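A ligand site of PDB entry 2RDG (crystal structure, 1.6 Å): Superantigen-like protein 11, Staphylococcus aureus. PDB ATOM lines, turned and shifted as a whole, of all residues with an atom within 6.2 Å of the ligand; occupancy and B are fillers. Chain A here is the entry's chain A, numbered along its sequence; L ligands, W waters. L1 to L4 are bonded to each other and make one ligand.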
ATOM      1  N   LEU A 130      -7.090  26.365   9.455  1.00  0.00           N
ATOM      2  CA  LEU A 130      -6.363  25.715  10.552  1.00  0.00           C
ATOM      3  C   LEU A 130      -5.466  26.741  11.251  1.00  0.00           C
ATOM      4  O   LEU A 130      -5.252  26.653  12.460  1.00  0.00           O
ATOM      5  CB  LEU A 130      -5.543  24.526  10.056  1.00  0.00           C
ATOM      6  CG  LEU A 130      -6.354  23.397   9.401  1.00  0.00           C
ATOM      7  CD1 LEU A 130      -5.422  22.215   9.122  1.00  0.00           C
ATOM      8  CD2 LEU A 130      -7.527  22.942  10.247  1.00  0.00           C
ATOM      9  N   ARG A 158      -6.972  18.324  19.163  1.00  0.00           N
ATOM     10  CA  ARG A 158      -7.588  17.618  18.039  1.00  0.00           C
ATOM     11  C   ARG A 158      -8.982  18.153  17.758  1.00  0.00           C
ATOM     12  O   ARG A 158      -9.849  18.171  18.653  1.00  0.00           O
ATOM     13  CB  ARG A 158      -7.611  16.093  18.264  1.00  0.00           C
ATOM     14  CG  ARG A 158      -8.204  15.341  17.077  1.00  0.00           C
ATOM     15  CD  ARG A 158      -7.754  13.892  17.064  1.00  0.00           C
ATOM     16  NE  ARG A 158      -6.331  13.770  16.733  1.00  0.00           N
ATOM     17  CZ  ARG A 158      -5.654  12.629  16.845  1.00  0.00           C
ATOM     18  NH1 ARG A 158      -6.263  11.515  17.271  1.00  0.00           N
ATOM     19  NH2 ARG A 158      -4.356  12.596  16.528  1.00  0.00           N
ATOM     20  N   ASP A 165     -13.496  12.730  10.347  1.00  0.00           N
ATOM     21  CA  ASP A 165     -12.166  13.267  10.002  1.00  0.00           C
ATOM     22  C   ASP A 165     -11.653  14.061  11.177  1.00  0.00           C
ATOM     23  O   ASP A 165     -12.440  14.593  11.976  1.00  0.00           O
ATOM     24  CB  ASP A 165     -12.245  14.233   8.823  1.00  0.00           C
ATOM     25  CG  ASP A 165     -12.497  13.549   7.479  1.00  0.00           C
ATOM     26  OD1 ASP A 165     -12.460  12.300   7.377  1.00  0.00           O
ATOM     27  OD2 ASP A 165     -12.720  14.320   6.521  1.00  0.00           O
ATOM     28  N   PHE A 166     -10.335  14.195  11.289  1.00  0.00           N
ATOM     29  CA  PHE A 166      -9.816  15.112  12.300  1.00  0.00           C
ATOM     30  C   PHE A 166      -8.544  15.825  11.873  1.00  0.00           C
ATOM     31  O   PHE A 166      -7.914  15.458  10.873  1.00  0.00           O
ATOM     32  CB  PHE A 166      -9.654  14.413  13.666  1.00  0.00           C
ATOM     33  CG  PHE A 166      -8.742  13.227  13.656  1.00  0.00           C
ATOM     34  CD1 PHE A 166      -7.357  13.378  13.552  1.00  0.00           C
ATOM     35  CD2 PHE A 166      -9.279  11.935  13.772  1.00  0.00           C
ATOM     36  CE1 PHE A 166      -6.511  12.266  13.567  1.00  0.00           C
ATOM     37  CE2 PHE A 166      -8.428  10.816  13.792  1.00  0.00           C
ATOM     38  CZ  PHE A 166      -7.050  10.989  13.685  1.00  0.00           C
ATOM     39  N   TYR A 167      -8.210  16.859  12.641  1.00  0.00           N
ATOM     40  CA  TYR A 167      -7.036  17.708  12.441  1.00  0.00           C
ATOM     41  C   TYR A 167      -6.357  17.912  13.768  1.00  0.00           C
ATOM     42  O   TYR A 167      -6.996  18.257  14.767  1.00  0.00           O
ATOM     43  CB  TYR A 167      -7.467  19.061  11.868  1.00  0.00           C
ATOM     44  CG  TYR A 167      -8.254  18.885  10.599  1.00  0.00           C
ATOM     45  CD1 TYR A 167      -9.646  18.766  10.619  1.00  0.00           C
ATOM     46  CD2 TYR A 167      -7.587  18.742   9.364  1.00  0.00           C
ATOM     47  CE1 TYR A 167     -10.373  18.569   9.449  1.00  0.00           C
ATOM     48  CE2 TYR A 167      -8.302  18.540   8.191  1.00  0.00           C
ATOM     49  CZ  TYR A 167      -9.695  18.438   8.244  1.00  0.00           C
ATOM     50  OH  TYR A 167     -10.380  18.234   7.071  1.00  0.00           O
ATOM     51  N   THR A 168      -5.047  17.684  13.786  1.00  0.00           N
ATOM     52  CA  THR A 168      -4.289  17.702  15.025  1.00  0.00           C
ATOM     53  C   THR A 168      -3.241  18.808  15.030  1.00  0.00           C
ATOM     54  O   THR A 168      -2.505  18.988  14.027  1.00  0.00           O
ATOM     55  CB  THR A 168      -3.542  16.356  15.226  1.00  0.00           C
ATOM     56  OG1 THR A 168      -4.470  15.263  15.143  1.00  0.00           O
ATOM     57  CG2 THR A 168      -2.848  16.320  16.587  1.00  0.00           C
ATOM     58  N   PHE A 169      -3.163  19.537  16.137  1.00  0.00           N
ATOM     59  CA  PHE A 169      -2.089  20.496  16.344  1.00  0.00           C
ATOM     60  C   PHE A 169      -1.240  20.018  17.511  1.00  0.00           C
ATOM     61  O   PHE A 169      -1.659  20.060  18.679  1.00  0.00           O
ATOM     62  CB  PHE A 169      -2.634  21.910  16.630  1.00  0.00           C
ATOM     63  CG  PHE A 169      -3.758  22.325  15.704  1.00  0.00           C
ATOM     64  CD1 PHE A 169      -3.687  22.084  14.332  1.00  0.00           C
ATOM     65  CD2 PHE A 169      -4.867  22.982  16.225  1.00  0.00           C
ATOM     66  CE1 PHE A 169      -4.717  22.480  13.482  1.00  0.00           C
ATOM     67  CE2 PHE A 169      -5.924  23.379  15.392  1.00  0.00           C
ATOM     68  CZ  PHE A 169      -5.847  23.131  14.023  1.00  0.00           C
ATOM     69  N   GLU A 170      -0.040  19.541  17.189  1.00  0.00           N
ATOM     70  CA  GLU A 170       0.881  19.096  18.235  1.00  0.00           C
ATOM     71  C   GLU A 170       1.452  20.334  18.909  1.00  0.00           C
ATOM     72  O   GLU A 170       2.007  21.228  18.237  1.00  0.00           O
ATOM     73  CB  GLU A 170       1.979  18.228  17.616  1.00  0.00           C
ATOM     74  CG  GLU A 170       1.447  16.914  17.121  1.00  0.00           C
ATOM     75  CD  GLU A 170       2.470  16.059  16.386  1.00  0.00           C
ATOM     76  OE1 GLU A 170       3.378  16.629  15.752  1.00  0.00           O
ATOM     77  OE2 GLU A 170       2.319  14.813  16.441  1.00  0.00           O
ATOM     78  N   ASN A 172       3.961  20.904  20.887  1.00  0.00           N
ATOM     79  CA  ASN A 172       5.420  21.061  21.077  1.00  0.00           C
ATOM     80  C   ASN A 172       6.113  21.622  19.830  1.00  0.00           C
ATOM     81  O   ASN A 172       7.353  21.698  19.760  1.00  0.00           O
ATOM     82  CB  ASN A 172       6.064  19.746  21.529  1.00  0.00           C
ATOM     83  CG  ASN A 172       6.057  18.692  20.448  1.00  0.00           C
ATOM     84  OD1 ASN A 172       5.641  18.927  19.321  1.00  0.00           O
ATOM     85  ND2 ASN A 172       6.547  17.492  20.804  1.00  0.00           N
ATOM     86  N   LYS A 173       5.308  22.030  18.849  1.00  0.00           N
ATOM     87  CA  LYS A 173       5.856  22.651  17.646  1.00  0.00           C
ATOM     88  C   LYS A 173       4.832  23.661  17.101  1.00  0.00           C
ATOM     89  O   LYS A 173       3.621  23.568  17.371  1.00  0.00           O
ATOM     90  CB  LYS A 173       6.196  21.584  16.580  1.00  0.00           C
ATOM     91  CG  LYS A 173       5.029  20.638  16.238  1.00  0.00           C
ATOM     92  CD  LYS A 173       5.416  19.623  15.147  1.00  0.00           C
ATOM     93  CE  LYS A 173       6.371  18.525  15.640  1.00  0.00           C
ATOM     94  NZ  LYS A 173       5.895  17.670  16.780  1.00  0.00           N
ATOM     95  N   LEU A 175       2.336  25.224  14.286  1.00  0.00           N
ATOM     96  CA  LEU A 175       1.615  24.658  13.137  1.00  0.00           C
ATOM     97  C   LEU A 175       2.540  24.763  11.928  1.00  0.00           C
ATOM     98  O   LEU A 175       3.123  25.812  11.676  1.00  0.00           O
ATOM     99  CB  LEU A 175       0.336  25.449  12.883  1.00  0.00           C
ATOM    100  CG  LEU A 175      -0.514  24.963  11.712  1.00  0.00           C
ATOM    101  CD1 LEU A 175      -1.017  23.529  11.954  1.00  0.00           C
ATOM    102  CD2 LEU A 175      -1.679  25.916  11.545  1.00  0.00           C
ATOM    103  N   GLN A 176       2.692  23.659  11.198  1.00  0.00           N
ATOM    104  CA  GLN A 176       3.569  23.667  10.015  1.00  0.00           C
ATOM    105  C   GLN A 176       3.077  24.712   9.005  1.00  0.00           C
ATOM    106  O   GLN A 176       1.861  24.847   8.765  1.00  0.00           O
ATOM    107  CB  GLN A 176       3.622  22.287   9.370  1.00  0.00           C
ATOM    108  CG  GLN A 176       4.248  21.195  10.228  1.00  0.00           C
ATOM    109  CD  GLN A 176       3.214  20.401  11.006  1.00  0.00           C
ATOM    110  OE1 GLN A 176       2.133  20.891  11.349  1.00  0.00           O
ATOM    111  NE2 GLN A 176       3.547  19.139  11.287  1.00  0.00           N
ATOM    112  N   HIS A 178       2.983  24.870   5.832  1.00  0.00           N
ATOM    113  CA  HIS A 178       2.209  24.370   4.676  1.00  0.00           C
ATOM    114  C   HIS A 178       0.781  23.979   5.020  1.00  0.00           C
ATOM    115  O   HIS A 178      -0.005  23.679   4.125  1.00  0.00           O
ATOM    116  CB  HIS A 178       2.929  23.198   4.010  1.00  0.00           C
ATOM    117  CG  HIS A 178       3.056  21.994   4.882  1.00  0.00           C
ATOM    118  ND1 HIS A 178       4.124  21.799   5.725  1.00  0.00           N
ATOM    119  CD2 HIS A 178       2.237  20.924   5.049  1.00  0.00           C
ATOM    120  CE1 HIS A 178       3.969  20.652   6.369  1.00  0.00           C
ATOM    121  NE2 HIS A 178       2.832  20.105   5.979  1.00  0.00           N
ATOM    122  N   ARG A 179       0.452  24.000   6.317  1.00  0.00           N
ATOM    123  CA  ARG A 179      -0.902  23.688   6.787  1.00  0.00           C
ATOM    124  C   ARG A 179      -1.710  24.937   7.123  1.00  0.00           C
ATOM    125  O   ARG A 179      -2.906  24.860   7.397  1.00  0.00           O
ATOM    126  CB  ARG A 179      -0.845  22.777   8.017  1.00  0.00           C
ATOM    127  CG  ARG A 179      -0.269  21.404   7.731  1.00  0.00           C
ATOM    128  CD  ARG A 179      -0.160  20.571   9.020  1.00  0.00           C
ATOM    129  NE  ARG A 179      -1.466  20.278   9.602  1.00  0.00           N
ATOM    130  CZ  ARG A 179      -1.673  20.034  10.907  1.00  0.00           C
ATOM    131  NH1 ARG A 179      -0.677  20.070  11.782  1.00  0.00           N
ATOM    132  NH2 ARG A 179      -2.904  19.767  11.325  1.00  0.00           N
ATOM    133  N   ASP A 182      -4.724  25.661   4.973  1.00  0.00           N
ATOM    134  CA  ASP A 182      -5.751  24.615   4.919  1.00  0.00           C
ATOM    135  C   ASP A 182      -7.027  25.108   5.574  1.00  0.00           C
ATOM    136  O   ASP A 182      -6.977  25.786   6.610  1.00  0.00           O
ATOM    137  CB  ASP A 182      -5.277  23.344   5.617  1.00  0.00           C
ATOM    138  CG  ASP A 182      -4.153  22.643   4.853  1.00  0.00           C
ATOM    139  OD1 ASP A 182      -3.875  23.006   3.697  1.00  0.00           O
ATOM    140  OD2 ASP A 182      -3.556  21.717   5.422  1.00  0.00           O
HETATM  141  C1  LIG L   1      -3.861  15.197  11.622  1.00  0.00           C
HETATM  142  C2  LIG L   1      -3.410  14.450  10.379  1.00  0.00           C
HETATM  143  C3  LIG L   1      -4.094  13.083  10.165  1.00  0.00           C
HETATM  144  C4  LIG L   1      -5.558  13.266   9.702  1.00  0.00           C
HETATM  145  C5  LIG L   1      -5.652  14.239   8.508  1.00  0.00           C
HETATM  146  C6  LIG L   1      -4.937  15.537   8.881  1.00  0.00           C
HETATM  147  C7  LIG L   1      -4.980  16.591   7.777  1.00  0.00           C
HETATM  148  C8  LIG L   1      -4.082  17.773   8.128  1.00  0.00           C
HETATM  149  C9  LIG L   1      -4.365  18.963   7.211  1.00  0.00           C
HETATM  150  C10 LIG L   1      -7.744  14.211   7.175  1.00  0.00           C
HETATM  151  C11 LIG L   1      -6.986  13.473   6.116  1.00  0.00           C
HETATM  152  N1  LIG L   1      -7.078  14.546   8.277  1.00  0.00           N
HETATM  153  O1  LIG L   1      -3.886  16.450  11.593  1.00  0.00           O
HETATM  154  O2  LIG L   1      -4.157  14.561  12.656  1.00  0.00           O
HETATM  155  O3  LIG L   1      -6.100  11.993   9.367  1.00  0.00           O
HETATM  156  O4  LIG L   1      -3.558  15.240   9.198  1.00  0.00           O
HETATM  157  O5  LIG L   1      -4.536  15.968   6.562  1.00  0.00           O
HETATM  158  O6  LIG L   1      -4.272  18.162   9.509  1.00  0.00           O
HETATM  159  O7  LIG L   1      -3.403  19.989   7.498  1.00  0.00           O
HETATM  160  O8  LIG L   1      -8.945  14.504   7.009  1.00  0.00           O
HETATM  161  C1  LG2 L   2       1.269  15.735   9.823  1.00  0.00           C
HETATM  162  C2  LG2 L   2       0.125  14.716   9.716  1.00  0.00           C
HETATM  163  C3  LG2 L   2      -1.063  15.152  10.561  1.00  0.00           C
HETATM  164  C4  LG2 L   2      -0.639  15.450  12.002  1.00  0.00           C
HETATM  165  C5  LG2 L   2       0.525  16.444  11.991  1.00  0.00           C
HETATM  166  C6  LG2 L   2       1.037  16.695  13.393  1.00  0.00           C
HETATM  167  O1  LG2 L   2      -0.311  14.568   8.377  1.00  0.00           O
HETATM  168  O2  LG2 L   2      -2.019  14.120  10.526  1.00  0.00           O
HETATM  169  O3  LG2 L   2      -0.277  14.220  12.612  1.00  0.00           O
HETATM  170  O4  LG2 L   2       1.615  15.985  11.172  1.00  0.00           O
HETATM  171  O5  LG2 L   2       2.075  17.643  13.387  1.00  0.00           O
HETATM  172  C1  LG3 L   3       5.402  16.688   6.647  1.00  0.00           C
HETATM  173  C2  LG3 L   3       5.717  16.547   8.133  1.00  0.00           C
HETATM  174  C3  LG3 L   3       4.718  15.670   8.866  1.00  0.00           C
HETATM  175  C4  LG3 L   3       3.282  16.130   8.565  1.00  0.00           C
HETATM  176  C5  LG3 L   3       3.105  16.208   7.042  1.00  0.00           C
HETATM  177  C6  LG3 L   3       1.696  16.648   6.646  1.00  0.00           C
HETATM  178  C7  LG3 L   3       8.063  16.764   8.760  1.00  0.00           C
HETATM  179  C8  LG3 L   3       9.391  16.066   8.857  1.00  0.00           C
HETATM  180  O1  LG3 L   3       4.048  17.117   6.494  1.00  0.00           O
HETATM  181  O2  LG3 L   3       4.918  15.699  10.267  1.00  0.00           O
HETATM  182  O3  LG3 L   3       2.388  15.171   9.105  1.00  0.00           O
HETATM  183  O4  LG3 L   3       1.417  17.944   7.155  1.00  0.00           O
HETATM  184  O5  LG3 L   3       7.959  17.949   9.096  1.00  0.00           O
HETATM  185  N1  LG3 L   3       7.058  16.009   8.287  1.00  0.00           N
HETATM  186  O6  LG3 L   3       5.602  15.452   5.987  1.00  0.00           O
HETATM  187  C1  LG4 L   4       5.626  14.549  10.786  1.00  0.00           C
HETATM  188  C2  LG4 L   4       6.103  14.879  12.203  1.00  0.00           C
HETATM  189  C3  LG4 L   4       4.893  14.924  13.149  1.00  0.00           C
HETATM  190  C4  LG4 L   4       4.067  13.631  13.043  1.00  0.00           C
HETATM  191  C5  LG4 L   4       3.691  13.363  11.586  1.00  0.00           C
HETATM  192  C6  LG4 L   4       2.909  12.065  11.408  1.00  0.00           C
HETATM  193  O1  LG4 L   4       6.796  16.114  12.230  1.00  0.00           O
HETATM  194  O2  LG4 L   4       5.308  15.164  14.478  1.00  0.00           O
HETATM  195  O3  LG4 L   4       4.775  12.519  13.601  1.00  0.00           O
HETATM  196  O4  LG4 L   4       4.874  13.333  10.776  1.00  0.00           O
HETATM  197  O   HOH W   1       4.005  12.656  16.297  1.00  0.00           O
HETATM  198  O   HOH W   2       9.331  16.532  13.149  1.00  0.00           O
HETATM  199  O   HOH W   3      10.323  19.277   9.512  1.00  0.00           O
HETATM  200  O   HOH W   4      -0.929  18.087   5.596  1.00  0.00           O
HETATM  201  O   HOH W   5       5.984  11.307   9.633  1.00  0.00           O
HETATM  202  O   HOH W   6       6.089  15.790   3.383  1.00  0.00           O
HETATM  203  O   HOH W   7       5.422   9.928  12.922  1.00  0.00           O
HETATM  204  O   HOH W   8       6.872  20.182   7.765  1.00  0.00           O
HETATM  205  O   HOH W   9       0.635  19.766  14.439  1.00  0.00           O
HETATM  206  O   HOH W  10      -2.487  12.462  13.324  1.00  0.00           O
HETATM  207  O   HOH W  11      -6.458  16.704   4.667  1.00  0.00           O
HETATM  208  O   HOH W  12       6.404  18.625  11.129  1.00  0.00           O
HETATM  209  O   HOH W  13      -1.800  15.579   6.374  1.00  0.00           O
HETATM  210  O   HOH W  14       7.441  14.014  15.457  1.00  0.00           O
HETATM  211  O   HOH W  15      -8.796  11.987   9.850  1.00  0.00           O
HETATM  212  O   HOH W  16       7.726  13.388   7.577  1.00  0.00           O
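Water W12 lies within hydrogen-bond range of an oxygen (O5) of LG3 L3 and the side-chain amide nitrogen (NE2) of Gln 176.
Water W15 bridges an oxygen (O3) of LIG L1 (2.7 Å) and the backbone NH (N) of Phe 166 (3.1 Å).
Water W9 lies within hydrogen-bond range of an oxygen (O5) of LG2 L2 (2.8 Å), the backbone NH (N) of Glu 170 (2.8 Å), the guanidinium group (NH1) of Arg 179 (3.0 Å) and the backbone carbonyl oxygen (O) of Thr 168 (3.3 Å).
Water W1 bridges OE2 of Glu 170 and O3 of LG4 L4.
An oxygen (O1) of LIG L1 is in hydrogen-bond range of the backbone NH (N) of Thr 168, at 2.8 Å.
OG1 of Thr 168 is in hydrogen-bond range of O2 of LIG L1 (2.6 Å).
O7 of LIG L1 is in hydrogen-bond range of OD2 of Asp 182 (2.7 Å).
O2 of LG4 L4 lies within hydrogen-bond range of OE1 of Glu 170.
An oxygen (O1) of LIG L1 lies within salt-bridge range of the guanidinium group of Arg 179 (3.5 Å).
NE2 of His 178 lies within hydrogen-bond range of O4 of LG3 L3.
The backbone carbonyl oxygen (O) of Phe 166 is in hydrogen-bond range of a nitrogen (N1) of LIG L1 (2.9 Å).
NE2 of Gln 176 lies within hydrogen-bond range of O5 of LG2 L2 (3.0 Å).
The side-chain amino group (NZ) of Lys 173 sits at hydrogen-bond distance from an oxygen (O2) of LG4 L4 (3.5 Å).
Merely in contact with the ligand: Tyr 167 (3.4 Å), Leu 130 (3.4 Å) and Asp 165 (3.7 Å).
Hydrophobic or aromatic side chains that line the ligand: Leu 130, Phe 166, Tyr 167 and His 178.
11 residues have an atom within 4 Å of the ligand: Leu 130, Asp 165, Phe 166, Tyr 167, Thr 168, Glu 170, Lys 173, Gln 176, His 178, Arg 179 and Asp 182.
NH2 of Arg 179 sits at hydrogen-bond distance from O of Thr 168.
OG1 of Thr 168 lies within hydrogen-bond range of NE of Arg 158.
The backbone carbonyl oxygen (O) of Asp 182 sits at hydrogen-bond distance from the backbone NH (N) of Leu 130, at 2.9 Å.
NZ of Lys 173 is in salt-bridge range of OE1 of Glu 170 (2.9 Å).
OE1 of Gln 176 lies within hydrogen-bond range of NH1 of Arg 179 (3.0 Å).
The side-chain amide oxygen (OD1) of Asn 172 is in hydrogen-bond range of the side-chain amino group (NZ) of Lys 173, 2.8 Å away.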
